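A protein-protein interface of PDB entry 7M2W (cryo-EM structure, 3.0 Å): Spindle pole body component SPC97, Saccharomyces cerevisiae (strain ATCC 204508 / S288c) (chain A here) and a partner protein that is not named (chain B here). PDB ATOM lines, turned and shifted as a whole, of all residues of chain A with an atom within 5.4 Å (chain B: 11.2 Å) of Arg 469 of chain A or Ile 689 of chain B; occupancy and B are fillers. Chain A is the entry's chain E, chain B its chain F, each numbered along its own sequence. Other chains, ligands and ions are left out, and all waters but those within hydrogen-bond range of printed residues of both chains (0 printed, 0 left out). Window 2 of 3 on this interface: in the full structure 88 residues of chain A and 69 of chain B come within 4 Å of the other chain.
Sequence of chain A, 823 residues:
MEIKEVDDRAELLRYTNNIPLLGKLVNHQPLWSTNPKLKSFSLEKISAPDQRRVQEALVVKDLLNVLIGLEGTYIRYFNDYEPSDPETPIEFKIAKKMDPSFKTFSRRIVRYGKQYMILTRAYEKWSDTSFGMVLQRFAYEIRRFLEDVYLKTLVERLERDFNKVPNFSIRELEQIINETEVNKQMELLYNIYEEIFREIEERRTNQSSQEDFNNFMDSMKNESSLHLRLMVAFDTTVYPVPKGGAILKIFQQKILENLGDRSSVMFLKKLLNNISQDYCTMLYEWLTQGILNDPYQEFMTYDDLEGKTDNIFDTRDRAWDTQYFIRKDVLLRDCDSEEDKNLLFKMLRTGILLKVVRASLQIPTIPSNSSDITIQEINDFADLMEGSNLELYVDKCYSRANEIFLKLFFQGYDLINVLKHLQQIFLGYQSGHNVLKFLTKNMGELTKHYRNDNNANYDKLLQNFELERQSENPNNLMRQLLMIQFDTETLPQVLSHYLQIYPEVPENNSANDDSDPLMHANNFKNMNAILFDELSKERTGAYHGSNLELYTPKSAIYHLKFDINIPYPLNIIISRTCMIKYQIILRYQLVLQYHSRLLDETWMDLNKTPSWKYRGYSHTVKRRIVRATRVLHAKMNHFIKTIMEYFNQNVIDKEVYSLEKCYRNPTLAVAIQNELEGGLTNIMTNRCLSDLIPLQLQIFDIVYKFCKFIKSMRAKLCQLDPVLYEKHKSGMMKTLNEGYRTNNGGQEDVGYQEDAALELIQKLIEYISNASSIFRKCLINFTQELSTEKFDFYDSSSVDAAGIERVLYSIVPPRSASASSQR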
ATOM      1  N   ASN A 464      -2.051 -23.499   8.465  1.00  0.00           N
ATOM      2  CA  ASN A 464      -1.407 -22.206   8.672  1.00  0.00           C
ATOM      3  C   ASN A 464      -2.435 -21.144   9.045  1.00  0.00           C
ATOM      4  O   ASN A 464      -2.187 -20.305   9.921  1.00  0.00           O
ATOM      5  CB  ASN A 464      -0.638 -21.793   7.417  1.00  0.00           C
ATOM      6  CG  ASN A 464       0.783 -22.323   7.402  1.00  0.00           C
ATOM      7  OD1 ASN A 464       1.180 -23.094   8.274  1.00  0.00           O
ATOM      8  ND2 ASN A 464       1.557 -21.911   6.405  1.00  0.00           N
ATOM      9  N   PHE A 465      -3.600 -21.175   8.395  1.00  0.00           N
ATOM     10  CA  PHE A 465      -4.653 -20.209   8.687  1.00  0.00           C
ATOM     11  C   PHE A 465      -5.112 -20.314  10.135  1.00  0.00           C
ATOM     12  O   PHE A 465      -5.177 -19.309  10.847  1.00  0.00           O
ATOM     13  CB  PHE A 465      -5.828 -20.409   7.727  1.00  0.00           C
ATOM     14  CG  PHE A 465      -6.959 -19.441   7.938  1.00  0.00           C
ATOM     15  CD1 PHE A 465      -7.027 -18.268   7.209  1.00  0.00           C
ATOM     16  CD2 PHE A 465      -7.969 -19.716   8.847  1.00  0.00           C
ATOM     17  CE1 PHE A 465      -8.066 -17.378   7.396  1.00  0.00           C
ATOM     18  CE2 PHE A 465      -9.008 -18.831   9.039  1.00  0.00           C
ATOM     19  CZ  PHE A 465      -9.059 -17.662   8.312  1.00  0.00           C
ATOM     20  N   GLU A 466      -5.460 -21.524  10.582  1.00  0.00           N
ATOM     21  CA  GLU A 466      -5.912 -21.686  11.959  1.00  0.00           C
ATOM     22  C   GLU A 466      -4.797 -21.370  12.949  1.00  0.00           C
ATOM     23  O   GLU A 466      -5.061 -20.892  14.057  1.00  0.00           O
ATOM     24  CB  GLU A 466      -6.477 -23.094  12.180  1.00  0.00           C
ATOM     25  CG  GLU A 466      -5.512 -24.251  11.954  1.00  0.00           C
ATOM     26  CD  GLU A 466      -4.621 -24.548  13.150  1.00  0.00           C
ATOM     27  OE1 GLU A 466      -4.876 -24.003  14.243  1.00  0.00           O
ATOM     28  OE2 GLU A 466      -3.665 -25.335  12.992  1.00  0.00           O
ATOM     29  N   LEU A 467      -3.539 -21.603  12.564  1.00  0.00           N
ATOM     30  CA  LEU A 467      -2.435 -21.241  13.445  1.00  0.00           C
ATOM     31  C   LEU A 467      -2.351 -19.731  13.630  1.00  0.00           C
ATOM     32  O   LEU A 467      -2.219 -19.248  14.761  1.00  0.00           O
ATOM     33  CB  LEU A 467      -1.119 -21.792  12.897  1.00  0.00           C
ATOM     34  CG  LEU A 467       0.101 -21.590  13.798  1.00  0.00           C
ATOM     35  CD1 LEU A 467       0.206 -22.713  14.819  1.00  0.00           C
ATOM     36  CD2 LEU A 467       1.371 -21.491  12.973  1.00  0.00           C
ATOM     37  N   GLU A 468      -2.414 -18.969  12.534  1.00  0.00           N
ATOM     38  CA  GLU A 468      -2.456 -17.513  12.665  1.00  0.00           C
ATOM     39  C   GLU A 468      -3.699 -17.067  13.427  1.00  0.00           C
ATOM     40  O   GLU A 468      -3.652 -16.092  14.187  1.00  0.00           O
ATOM     41  CB  GLU A 468      -2.403 -16.837  11.293  1.00  0.00           C
ATOM     42  CG  GLU A 468      -1.409 -17.428  10.304  1.00  0.00           C
ATOM     43  CD  GLU A 468      -0.052 -17.717  10.917  1.00  0.00           C
ATOM     44  OE1 GLU A 468       0.449 -18.850  10.748  1.00  0.00           O
ATOM     45  OE2 GLU A 468       0.520 -16.812  11.560  1.00  0.00           O
ATOM     46  N   ARG A 469      -4.816 -17.768  13.233  1.00  0.00           N
ATOM     47  CA  ARG A 469      -6.047 -17.434  13.943  1.00  0.00           C
ATOM     48  C   ARG A 469      -5.895 -17.649  15.442  1.00  0.00           C
ATOM     49  O   ARG A 469      -6.535 -16.965  16.246  1.00  0.00           O
ATOM     50  CB  ARG A 469      -7.202 -18.271  13.391  1.00  0.00           C
ATOM     51  CG  ARG A 469      -8.583 -17.738  13.715  1.00  0.00           C
ATOM     52  CD  ARG A 469      -9.615 -18.270  12.733  1.00  0.00           C
ATOM     53  NE  ARG A 469      -9.846 -19.701  12.896  1.00  0.00           N
ATOM     54  CZ  ARG A 469     -10.629 -20.230  13.829  1.00  0.00           C
ATOM     55  NH1 ARG A 469     -11.260 -19.446  14.691  1.00  0.00           N
ATOM     56  NH2 ARG A 469     -10.781 -21.545  13.902  1.00  0.00           N
ATOM     57  N   GLN A 470      -5.054 -18.609  15.834  1.00  0.00           N
ATOM     58  CA  GLN A 470      -4.749 -18.799  17.247  1.00  0.00           C
ATOM     59  C   GLN A 470      -4.070 -17.578  17.851  1.00  0.00           C
ATOM     60  O   GLN A 470      -4.169 -17.361  19.063  1.00  0.00           O
ATOM     61  CB  GLN A 470      -3.864 -20.034  17.439  1.00  0.00           C
ATOM     62  CG  GLN A 470      -4.563 -21.352  17.152  1.00  0.00           C
ATOM     63  CD  GLN A 470      -4.245 -22.416  18.183  1.00  0.00           C
ATOM     64  OE1 GLN A 470      -4.160 -22.133  19.377  1.00  0.00           O
ATOM     65  NE2 GLN A 470      -4.068 -23.651  17.725  1.00  0.00           N
ATOM     66  N   SER A 471      -3.388 -16.776  17.035  1.00  0.00           N
ATOM     67  CA  SER A 471      -2.746 -15.552  17.484  1.00  0.00           C
ATOM     68  C   SER A 471      -3.624 -14.324  17.299  1.00  0.00           C
ATOM     69  O   SER A 471      -3.133 -13.200  17.442  1.00  0.00           O
ATOM     70  CB  SER A 471      -1.420 -15.350  16.744  1.00  0.00           C
ATOM     71  OG  SER A 471      -1.642 -14.933  15.409  1.00  0.00           O
ATOM     72  N   GLU A 472      -4.901 -14.509  16.980  1.00  0.00           N
ATOM     73  CA  GLU A 472      -5.797 -13.386  16.763  1.00  0.00           C
ATOM     74  C   GLU A 472      -6.407 -12.924  18.081  1.00  0.00           C
ATOM     75  O   GLU A 472      -6.256 -13.568  19.122  1.00  0.00           O
ATOM     76  CB  GLU A 472      -6.900 -13.764  15.773  1.00  0.00           C
ATOM     77  CG  GLU A 472      -7.412 -12.603  14.941  1.00  0.00           C
ATOM     78  CD  GLU A 472      -6.371 -12.070  13.979  1.00  0.00           C
ATOM     79  OE1 GLU A 472      -5.976 -12.812  13.057  1.00  0.00           O
ATOM     80  OE2 GLU A 472      -5.951 -10.906  14.144  1.00  0.00           O
ATOM     81  N   ARG A 479     -13.228 -12.667  13.135  1.00  0.00           N
ATOM     82  CA  ARG A 479     -12.073 -13.444  12.706  1.00  0.00           C
ATOM     83  C   ARG A 479     -12.070 -14.836  13.322  1.00  0.00           C
ATOM     84  O   ARG A 479     -11.680 -15.798  12.654  1.00  0.00           O
ATOM     85  CB  ARG A 479     -10.781 -12.700  13.039  1.00  0.00           C
ATOM     86  CG  ARG A 479     -10.577 -11.462  12.181  1.00  0.00           C
ATOM     87  CD  ARG A 479      -9.176 -10.901  12.311  1.00  0.00           C
ATOM     88  NE  ARG A 479      -8.974  -9.767  11.417  1.00  0.00           N
ATOM     89  CZ  ARG A 479      -8.616  -9.877  10.143  1.00  0.00           C
ATOM     90  NH1 ARG A 479      -8.417 -11.074   9.610  1.00  0.00           N
ATOM     91  NH2 ARG A 479      -8.454  -8.790   9.404  1.00  0.00           N
ATOM     92  N   GLN A 480     -12.491 -14.960  14.585  1.00  0.00           N
ATOM     93  CA  GLN A 480     -12.678 -16.280  15.182  1.00  0.00           C
ATOM     94  C   GLN A 480     -13.583 -17.165  14.334  1.00  0.00           C
ATOM     95  O   GLN A 480     -13.442 -18.392  14.351  1.00  0.00           O
ATOM     96  CB  GLN A 480     -13.260 -16.149  16.590  1.00  0.00           C
ATOM     97  CG  GLN A 480     -12.515 -15.194  17.503  1.00  0.00           C
ATOM     98  CD  GLN A 480     -11.271 -15.811  18.106  1.00  0.00           C
ATOM     99  OE1 GLN A 480     -10.984 -16.989  17.895  1.00  0.00           O
ATOM    100  NE2 GLN A 480     -10.528 -15.017  18.867  1.00  0.00           N
ATOM    101  N   LEU A 481     -14.506 -16.568  13.585  1.00  0.00           N
ATOM    102  CA  LEU A 481     -15.444 -17.316  12.763  1.00  0.00           C
ATOM    103  C   LEU A 481     -15.061 -17.330  11.292  1.00  0.00           C
ATOM    104  O   LEU A 481     -15.762 -17.954  10.491  1.00  0.00           O
ATOM    105  CB  LEU A 481     -16.855 -16.738  12.910  1.00  0.00           C
ATOM    106  CG  LEU A 481     -17.470 -16.746  14.308  1.00  0.00           C
ATOM    107  CD1 LEU A 481     -18.755 -15.941  14.317  1.00  0.00           C
ATOM    108  CD2 LEU A 481     -17.728 -18.164  14.776  1.00  0.00           C
ATOM    109  N   LEU A 482     -13.975 -16.661  10.920  1.00  0.00           N
ATOM    110  CA  LEU A 482     -13.572 -16.617   9.523  1.00  0.00           C
ATOM    111  C   LEU A 482     -13.102 -17.991   9.065  1.00  0.00           C
ATOM    112  O   LEU A 482     -12.090 -18.507   9.548  1.00  0.00           O
ATOM    113  CB  LEU A 482     -12.465 -15.586   9.326  1.00  0.00           C
ATOM    114  CG  LEU A 482     -12.053 -15.343   7.876  1.00  0.00           C
ATOM    115  CD1 LEU A 482     -13.196 -14.722   7.100  1.00  0.00           C
ATOM    116  CD2 LEU A 482     -10.824 -14.459   7.820  1.00  0.00           C
ATOM    117  N   MET A 483     -13.845 -18.585   8.139  1.00  0.00           N
ATOM    118  CA  MET A 483     -13.523 -19.891   7.586  1.00  0.00           C
ATOM    119  C   MET A 483     -12.906 -19.725   6.206  1.00  0.00           C
ATOM    120  O   MET A 483     -13.563 -19.246   5.277  1.00  0.00           O
ATOM    121  CB  MET A 483     -14.768 -20.775   7.491  1.00  0.00           C
ATOM    122  CG  MET A 483     -15.721 -20.637   8.662  1.00  0.00           C
ATOM    123  SD  MET A 483     -16.889 -22.004   8.762  1.00  0.00           S
ATOM    124  CE  MET A 483     -17.399 -22.151   7.054  1.00  0.00           C
ATOM    125  N   ASN A 565     -20.058 -17.578   9.095  1.00  0.00           N
ATOM    126  CA  ASN A 565     -21.421 -17.931   9.479  1.00  0.00           C
ATOM    127  C   ASN A 565     -21.868 -16.908  10.516  1.00  0.00           C
ATOM    128  O   ASN A 565     -21.757 -17.111  11.727  1.00  0.00           O
ATOM    129  CB  ASN A 565     -21.490 -19.355  10.015  1.00  0.00           C
ATOM    130  CG  ASN A 565     -21.389 -20.393   8.922  1.00  0.00           C
ATOM    131  OD1 ASN A 565     -21.802 -20.160   7.787  1.00  0.00           O
ATOM    132  ND2 ASN A 565     -20.839 -21.552   9.258  1.00  0.00           N
ATOM    133  N   ASN B 677     -13.084 -15.649  27.056  1.00  0.00           N
ATOM    134  CA  ASN B 677     -13.046 -16.430  25.821  1.00  0.00           C
ATOM    135  C   ASN B 677     -14.399 -17.128  25.712  1.00  0.00           C
ATOM    136  O   ASN B 677     -14.516 -18.356  25.714  1.00  0.00           O
ATOM    137  CB  ASN B 677     -11.873 -17.405  25.839  1.00  0.00           C
ATOM    138  CG  ASN B 677     -11.764 -18.236  24.570  1.00  0.00           C
ATOM    139  OD1 ASN B 677     -12.584 -18.123  23.658  1.00  0.00           O
ATOM    140  ND2 ASN B 677     -10.741 -19.082  24.509  1.00  0.00           N
ATOM    141  N   PHE B 679     -16.771 -17.246  23.381  1.00  0.00           N
ATOM    142  CA  PHE B 679     -17.352 -17.678  22.113  1.00  0.00           C
ATOM    143  C   PHE B 679     -17.290 -19.200  22.037  1.00  0.00           C
ATOM    144  O   PHE B 679     -16.303 -19.802  21.607  1.00  0.00           O
ATOM    145  CB  PHE B 679     -16.633 -17.016  20.946  1.00  0.00           C
ATOM    146  CG  PHE B 679     -16.558 -15.523  21.057  1.00  0.00           C
ATOM    147  CD1 PHE B 679     -15.400 -14.845  20.722  1.00  0.00           C
ATOM    148  CD2 PHE B 679     -17.645 -14.796  21.514  1.00  0.00           C
ATOM    149  CE1 PHE B 679     -15.332 -13.474  20.831  1.00  0.00           C
ATOM    150  CE2 PHE B 679     -17.580 -13.425  21.625  1.00  0.00           C
ATOM    151  CZ  PHE B 679     -16.423 -12.763  21.284  1.00  0.00           C
ATOM    152  N   ASP B 680     -18.376 -19.832  22.479  1.00  0.00           N
ATOM    153  CA  ASP B 680     -18.488 -21.290  22.469  1.00  0.00           C
ATOM    154  C   ASP B 680     -18.766 -21.753  21.044  1.00  0.00           C
ATOM    155  O   ASP B 680     -19.895 -22.064  20.669  1.00  0.00           O
ATOM    156  CB  ASP B 680     -19.552 -21.760  23.459  1.00  0.00           C
ATOM    157  CG  ASP B 680     -20.898 -21.080  23.257  1.00  0.00           C
ATOM    158  OD1 ASP B 680     -20.993 -20.161  22.421  1.00  0.00           O
ATOM    159  OD2 ASP B 680     -21.869 -21.472  23.939  1.00  0.00           O
ATOM    160  N   LEU B 681     -17.712 -21.797  20.239  1.00  0.00           N
ATOM    161  CA  LEU B 681     -17.812 -22.196  18.843  1.00  0.00           C
ATOM    162  C   LEU B 681     -18.178 -23.668  18.725  1.00  0.00           C
ATOM    163  O   LEU B 681     -17.968 -24.458  19.649  1.00  0.00           O
ATOM    164  CB  LEU B 681     -16.493 -21.932  18.116  1.00  0.00           C
ATOM    165  CG  LEU B 681     -16.315 -20.584  17.421  1.00  0.00           C
ATOM    166  CD1 LEU B 681     -16.675 -19.437  18.342  1.00  0.00           C
ATOM    167  CD2 LEU B 681     -14.880 -20.444  16.951  1.00  0.00           C
ATOM    168  N   ILE B 682     -18.735 -24.030  17.574  1.00  0.00           N
ATOM    169  CA  ILE B 682     -19.045 -25.414  17.243  1.00  0.00           C
ATOM    170  C   ILE B 682     -18.259 -25.793  15.999  1.00  0.00           C
ATOM    171  O   ILE B 682     -18.547 -25.302  14.901  1.00  0.00           O
ATOM    172  CB  ILE B 682     -20.551 -25.618  17.010  1.00  0.00           C
ATOM    173  CG1 ILE B 682     -21.342 -25.433  18.301  1.00  0.00           C
ATOM    174  CG2 ILE B 682     -20.817 -27.002  16.456  1.00  0.00           C
ATOM    175  CD1 ILE B 682     -22.834 -25.575  18.096  1.00  0.00           C
ATOM    176  N   ARG B 683     -17.270 -26.663  16.164  1.00  0.00           N
ATOM    177  CA  ARG B 683     -16.469 -27.141  15.048  1.00  0.00           C
ATOM    178  C   ARG B 683     -17.118 -28.375  14.438  1.00  0.00           C
ATOM    179  O   ARG B 683     -17.468 -29.321  15.149  1.00  0.00           O
ATOM    180  CB  ARG B 683     -15.043 -27.465  15.496  1.00  0.00           C
ATOM    181  CG  ARG B 683     -14.364 -26.350  16.278  1.00  0.00           C
ATOM    182  CD  ARG B 683     -14.196 -25.086  15.448  1.00  0.00           C
ATOM    183  NE  ARG B 683     -13.964 -25.367  14.034  1.00  0.00           N
ATOM    184  CZ  ARG B 683     -12.763 -25.535  13.494  1.00  0.00           C
ATOM    185  NH1 ARG B 683     -11.678 -25.449  14.250  1.00  0.00           N
ATOM    186  NH2 ARG B 683     -12.646 -25.786  12.197  1.00  0.00           N
ATOM    187  N   LEU B 684     -17.273 -28.362  13.120  1.00  0.00           N
ATOM    188  CA  LEU B 684     -17.860 -29.473  12.388  1.00  0.00           C
ATOM    189  C   LEU B 684     -16.775 -30.228  11.633  1.00  0.00           C
ATOM    190  O   LEU B 684     -15.736 -29.670  11.270  1.00  0.00           O
ATOM    191  CB  LEU B 684     -18.938 -28.996  11.406  1.00  0.00           C
ATOM    192  CG  LEU B 684     -20.352 -28.673  11.904  1.00  0.00           C
ATOM    193  CD1 LEU B 684     -20.350 -27.590  12.970  1.00  0.00           C
ATOM    194  CD2 LEU B 684     -21.258 -28.288  10.741  1.00  0.00           C
ATOM    195  N   ASN B 685     -17.032 -31.517  11.401  1.00  0.00           N
ATOM    196  CA  ASN B 685     -16.063 -32.372  10.727  1.00  0.00           C
ATOM    197  C   ASN B 685     -15.772 -31.936   9.297  1.00  0.00           C
ATOM    198  O   ASN B 685     -14.711 -32.285   8.768  1.00  0.00           O
ATOM    199  CB  ASN B 685     -16.549 -33.823  10.739  1.00  0.00           C
ATOM    200  CG  ASN B 685     -18.030 -33.945  10.445  1.00  0.00           C
ATOM    201  OD1 ASN B 685     -18.655 -33.012   9.940  1.00  0.00           O
ATOM    202  ND2 ASN B 685     -18.603 -35.100  10.762  1.00  0.00           N
ATOM    203  N   ASN B 686     -16.673 -31.190   8.661  1.00  0.00           N
ATOM    204  CA  ASN B 686     -16.441 -30.669   7.322  1.00  0.00           C
ATOM    205  C   ASN B 686     -15.668 -29.356   7.327  1.00  0.00           C
ATOM    206  O   ASN B 686     -15.465 -28.766   6.261  1.00  0.00           O
ATOM    207  CB  ASN B 686     -17.772 -30.494   6.583  1.00  0.00           C
ATOM    208  CG  ASN B 686     -18.797 -29.726   7.396  1.00  0.00           C
ATOM    209  OD1 ASN B 686     -18.451 -28.983   8.311  1.00  0.00           O
ATOM    210  ND2 ASN B 686     -20.069 -29.905   7.062  1.00  0.00           N
ATOM    211  N   GLY B 687     -15.239 -28.886   8.498  1.00  0.00           N
ATOM    212  CA  GLY B 687     -14.499 -27.650   8.612  1.00  0.00           C
ATOM    213  C   GLY B 687     -15.334 -26.426   8.911  1.00  0.00           C
ATOM    214  O   GLY B 687     -14.829 -25.303   8.781  1.00  0.00           O
ATOM    215  N   THR B 688     -16.593 -26.600   9.305  1.00  0.00           N
ATOM    216  CA  THR B 688     -17.475 -25.461   9.518  1.00  0.00           C
ATOM    217  C   THR B 688     -17.283 -24.879  10.913  1.00  0.00           C
ATOM    218  O   THR B 688     -16.971 -25.596  11.868  1.00  0.00           O
ATOM    219  CB  THR B 688     -18.932 -25.879   9.319  1.00  0.00           C
ATOM    220  OG1 THR B 688     -19.022 -26.780   8.209  1.00  0.00           O
ATOM    221  CG2 THR B 688     -19.800 -24.669   9.039  1.00  0.00           C
ATOM    222  N   ILE B 689     -17.469 -23.567  11.024  1.00  0.00           N
ATOM    223  CA  ILE B 689     -17.408 -22.854  12.294  1.00  0.00           C
ATOM    224  C   ILE B 689     -18.722 -22.105  12.467  1.00  0.00           C
ATOM    225  O   ILE B 689     -19.138 -21.357  11.574  1.00  0.00           O
ATOM    226  CB  ILE B 689     -16.215 -21.889  12.349  1.00  0.00           C
ATOM    227  CG1 ILE B 689     -14.918 -22.607  11.977  1.00  0.00           C
ATOM    228  CG2 ILE B 689     -16.106 -21.268  13.721  1.00  0.00           C
ATOM    229  CD1 ILE B 689     -13.692 -21.723  12.053  1.00  0.00           C
ATOM    230  N   GLU B 690     -19.373 -22.300  13.611  1.00  0.00           N
ATOM    231  CA  GLU B 690     -20.626 -21.625  13.908  1.00  0.00           C
ATOM    232  C   GLU B 690     -20.807 -21.531  15.415  1.00  0.00           C
ATOM    233  O   GLU B 690     -20.614 -22.508  16.141  1.00  0.00           O
ATOM    234  CB  GLU B 690     -21.824 -22.346  13.277  1.00  0.00           C
ATOM    235  CG  GLU B 690     -23.166 -21.691  13.566  1.00  0.00           C
ATOM    236  CD  GLU B 690     -24.288 -22.697  13.734  1.00  0.00           C
ATOM    237  OE1 GLU B 690     -25.322 -22.341  14.336  1.00  0.00           O
ATOM    238  OE2 GLU B 690     -24.135 -23.844  13.265  1.00  0.00           O
ATOM    239  N   LEU B 691     -21.181 -20.342  15.876  1.00  0.00           N
ATOM    240  CA  LEU B 691     -21.353 -20.105  17.302  1.00  0.00           C
ATOM    241  C   LEU B 691     -22.503 -20.945  17.846  1.00  0.00           C
ATOM    242  O   LEU B 691     -23.468 -21.239  17.138  1.00  0.00           O
ATOM    243  CB  LEU B 691     -21.610 -18.620  17.553  1.00  0.00           C
ATOM    244  CG  LEU B 691     -21.810 -18.139  18.987  1.00  0.00           C
ATOM    245  CD1 LEU B 691     -20.600 -18.497  19.814  1.00  0.00           C
ATOM    246  CD2 LEU B 691     -22.046 -16.644  19.016  1.00  0.00           C
ATOM    247  N   ASN B 692     -22.388 -21.345  19.113  1.00  0.00           N
ATOM    248  CA  ASN B 692     -23.429 -22.118  19.784  1.00  0.00           C
ATOM    249  C   ASN B 692     -24.524 -21.179  20.270  1.00  0.00           C
ATOM    250  O   ASN B 692     -24.282 -20.315  21.118  1.00  0.00           O
ATOM    251  CB  ASN B 692     -22.851 -22.912  20.951  1.00  0.00           C
ATOM    252  CG  ASN B 692     -23.477 -24.283  21.090  1.00  0.00           C
ATOM    253  OD1 ASN B 692     -24.601 -24.512  20.641  1.00  0.00           O
ATOM    254  ND2 ASN B 692     -22.754 -25.205  21.713  1.00  0.00           N
ATOM    255  N   GLY B 693     -25.726 -21.344  19.735  1.00  0.00           N
ATOM    256  CA  GLY B 693     -26.857 -20.571  20.193  1.00  0.00           C
ATOM    257  C   GLY B 693     -26.894 -19.181  19.591  1.00  0.00           C
ATOM    258  O   GLY B 693     -26.561 -18.951  18.425  1.00  0.00           O
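The side-chain sulfur of Met 483 of chain A lies within hydrogen-bond range of the backbone NH of Ile 689 of chain B (2.8 Å). The side-chain amide nitrogen (ND2) of Asn 565 of chain A is in hydrogen-bond range of the backbone carbonyl oxygen (O) of Ile 689 of chain B, at 2.9 Å.
The side-chain amide oxygen (OD1) of Asn 686 of chain B is in hydrogen-bond range of the backbone NH (N) of Thr 688 of chain B. The guanidinium group (NH1) of Arg 469 of chain A lies within hydrogen-bond range of the backbone carbonyl oxygen (O) of Gln 480 of chain A.
CD1 of Ile 689 of chain B touches NH2 of Arg 469 of chain A, at 3.5 Å. Leu 681 of chain B touches Gln 480 of chain A. O of Gln 480 of chain A touches CG2 of Ile 689 of chain B, at 3.97 Å. Leu 681 of chain B touches Leu 481 of chain A (CG to CD2, 3.9 Å). Leu 481 of chain A touches Ile 689 of chain B (CD2 to CG2, 3.7 Å). Gly 687 of chain B touches Met 483 of chain A. Thr 688 of chain B touches Met 483 of chain A. Asn 565 of chain A touches Thr 688 of chain B.
Arg 469 of chain A touches just one residue of chain B: Ile 689. Of chain A, only Arg 469, Gln 480, Leu 481, Met 483 and Asn 565 come within 4 Å of Ile 689 of chain B. No residue of chain B comes within 4 Å of Phe 465 of chain A. No residue of chain B comes within 4 Å of Gln 470 of chain A. No residue of chain B comes within 4 Å of Ser 471 of chain A. No residue of chain B comes within 4 Å of Glu 472 of chain A. Of chain B, only Leu 681 and Ile 689 come within 4 Å of Gln 480 of chain A. Leu 481 of chain A touches just these residues of chain B: Leu 681 (3.9 Å) and Ile 689 (3.7 Å). Asn 565 of chain A touches just these residues of chain B: Thr 688 (3.3 Å) and Ile 689 (2.9 Å). Of the printed residues of chain A, Thr 688 of chain B touches Met 483 and Asn 565. Of the printed residues of chain A, Leu 681 of chain B touches Gln 480 (3.6 Å) and Leu 481 (3.9 Å). Asn 464 of chain A touches none of the printed residues of chain B. Glu 466 of chain A touches none of the printed residues of chain B. The nearest residue of chain B that does not touch Arg 469 of chain A is Arg 683 of chain B (4.02 Å). The nearest residue of chain A that does not touch Ile 689 of chain B is Leu 482 of chain A (4.4 Å). The nearest printed residue of chain A that does not touch Gly 687 of chain B is Asn 565 of chain A (7.1 Å).
Of the 15 printed residues of chain A, 5 touch a printed residue of chain B. Hydrophobic or aromatic side chains of chain A within 4 Å of the printed part of chain B: Leu 481 and Met 483. Hydrophobic or aromatic side chains of chain B that line the printed part of chain A: Leu 681 and Ile 689.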
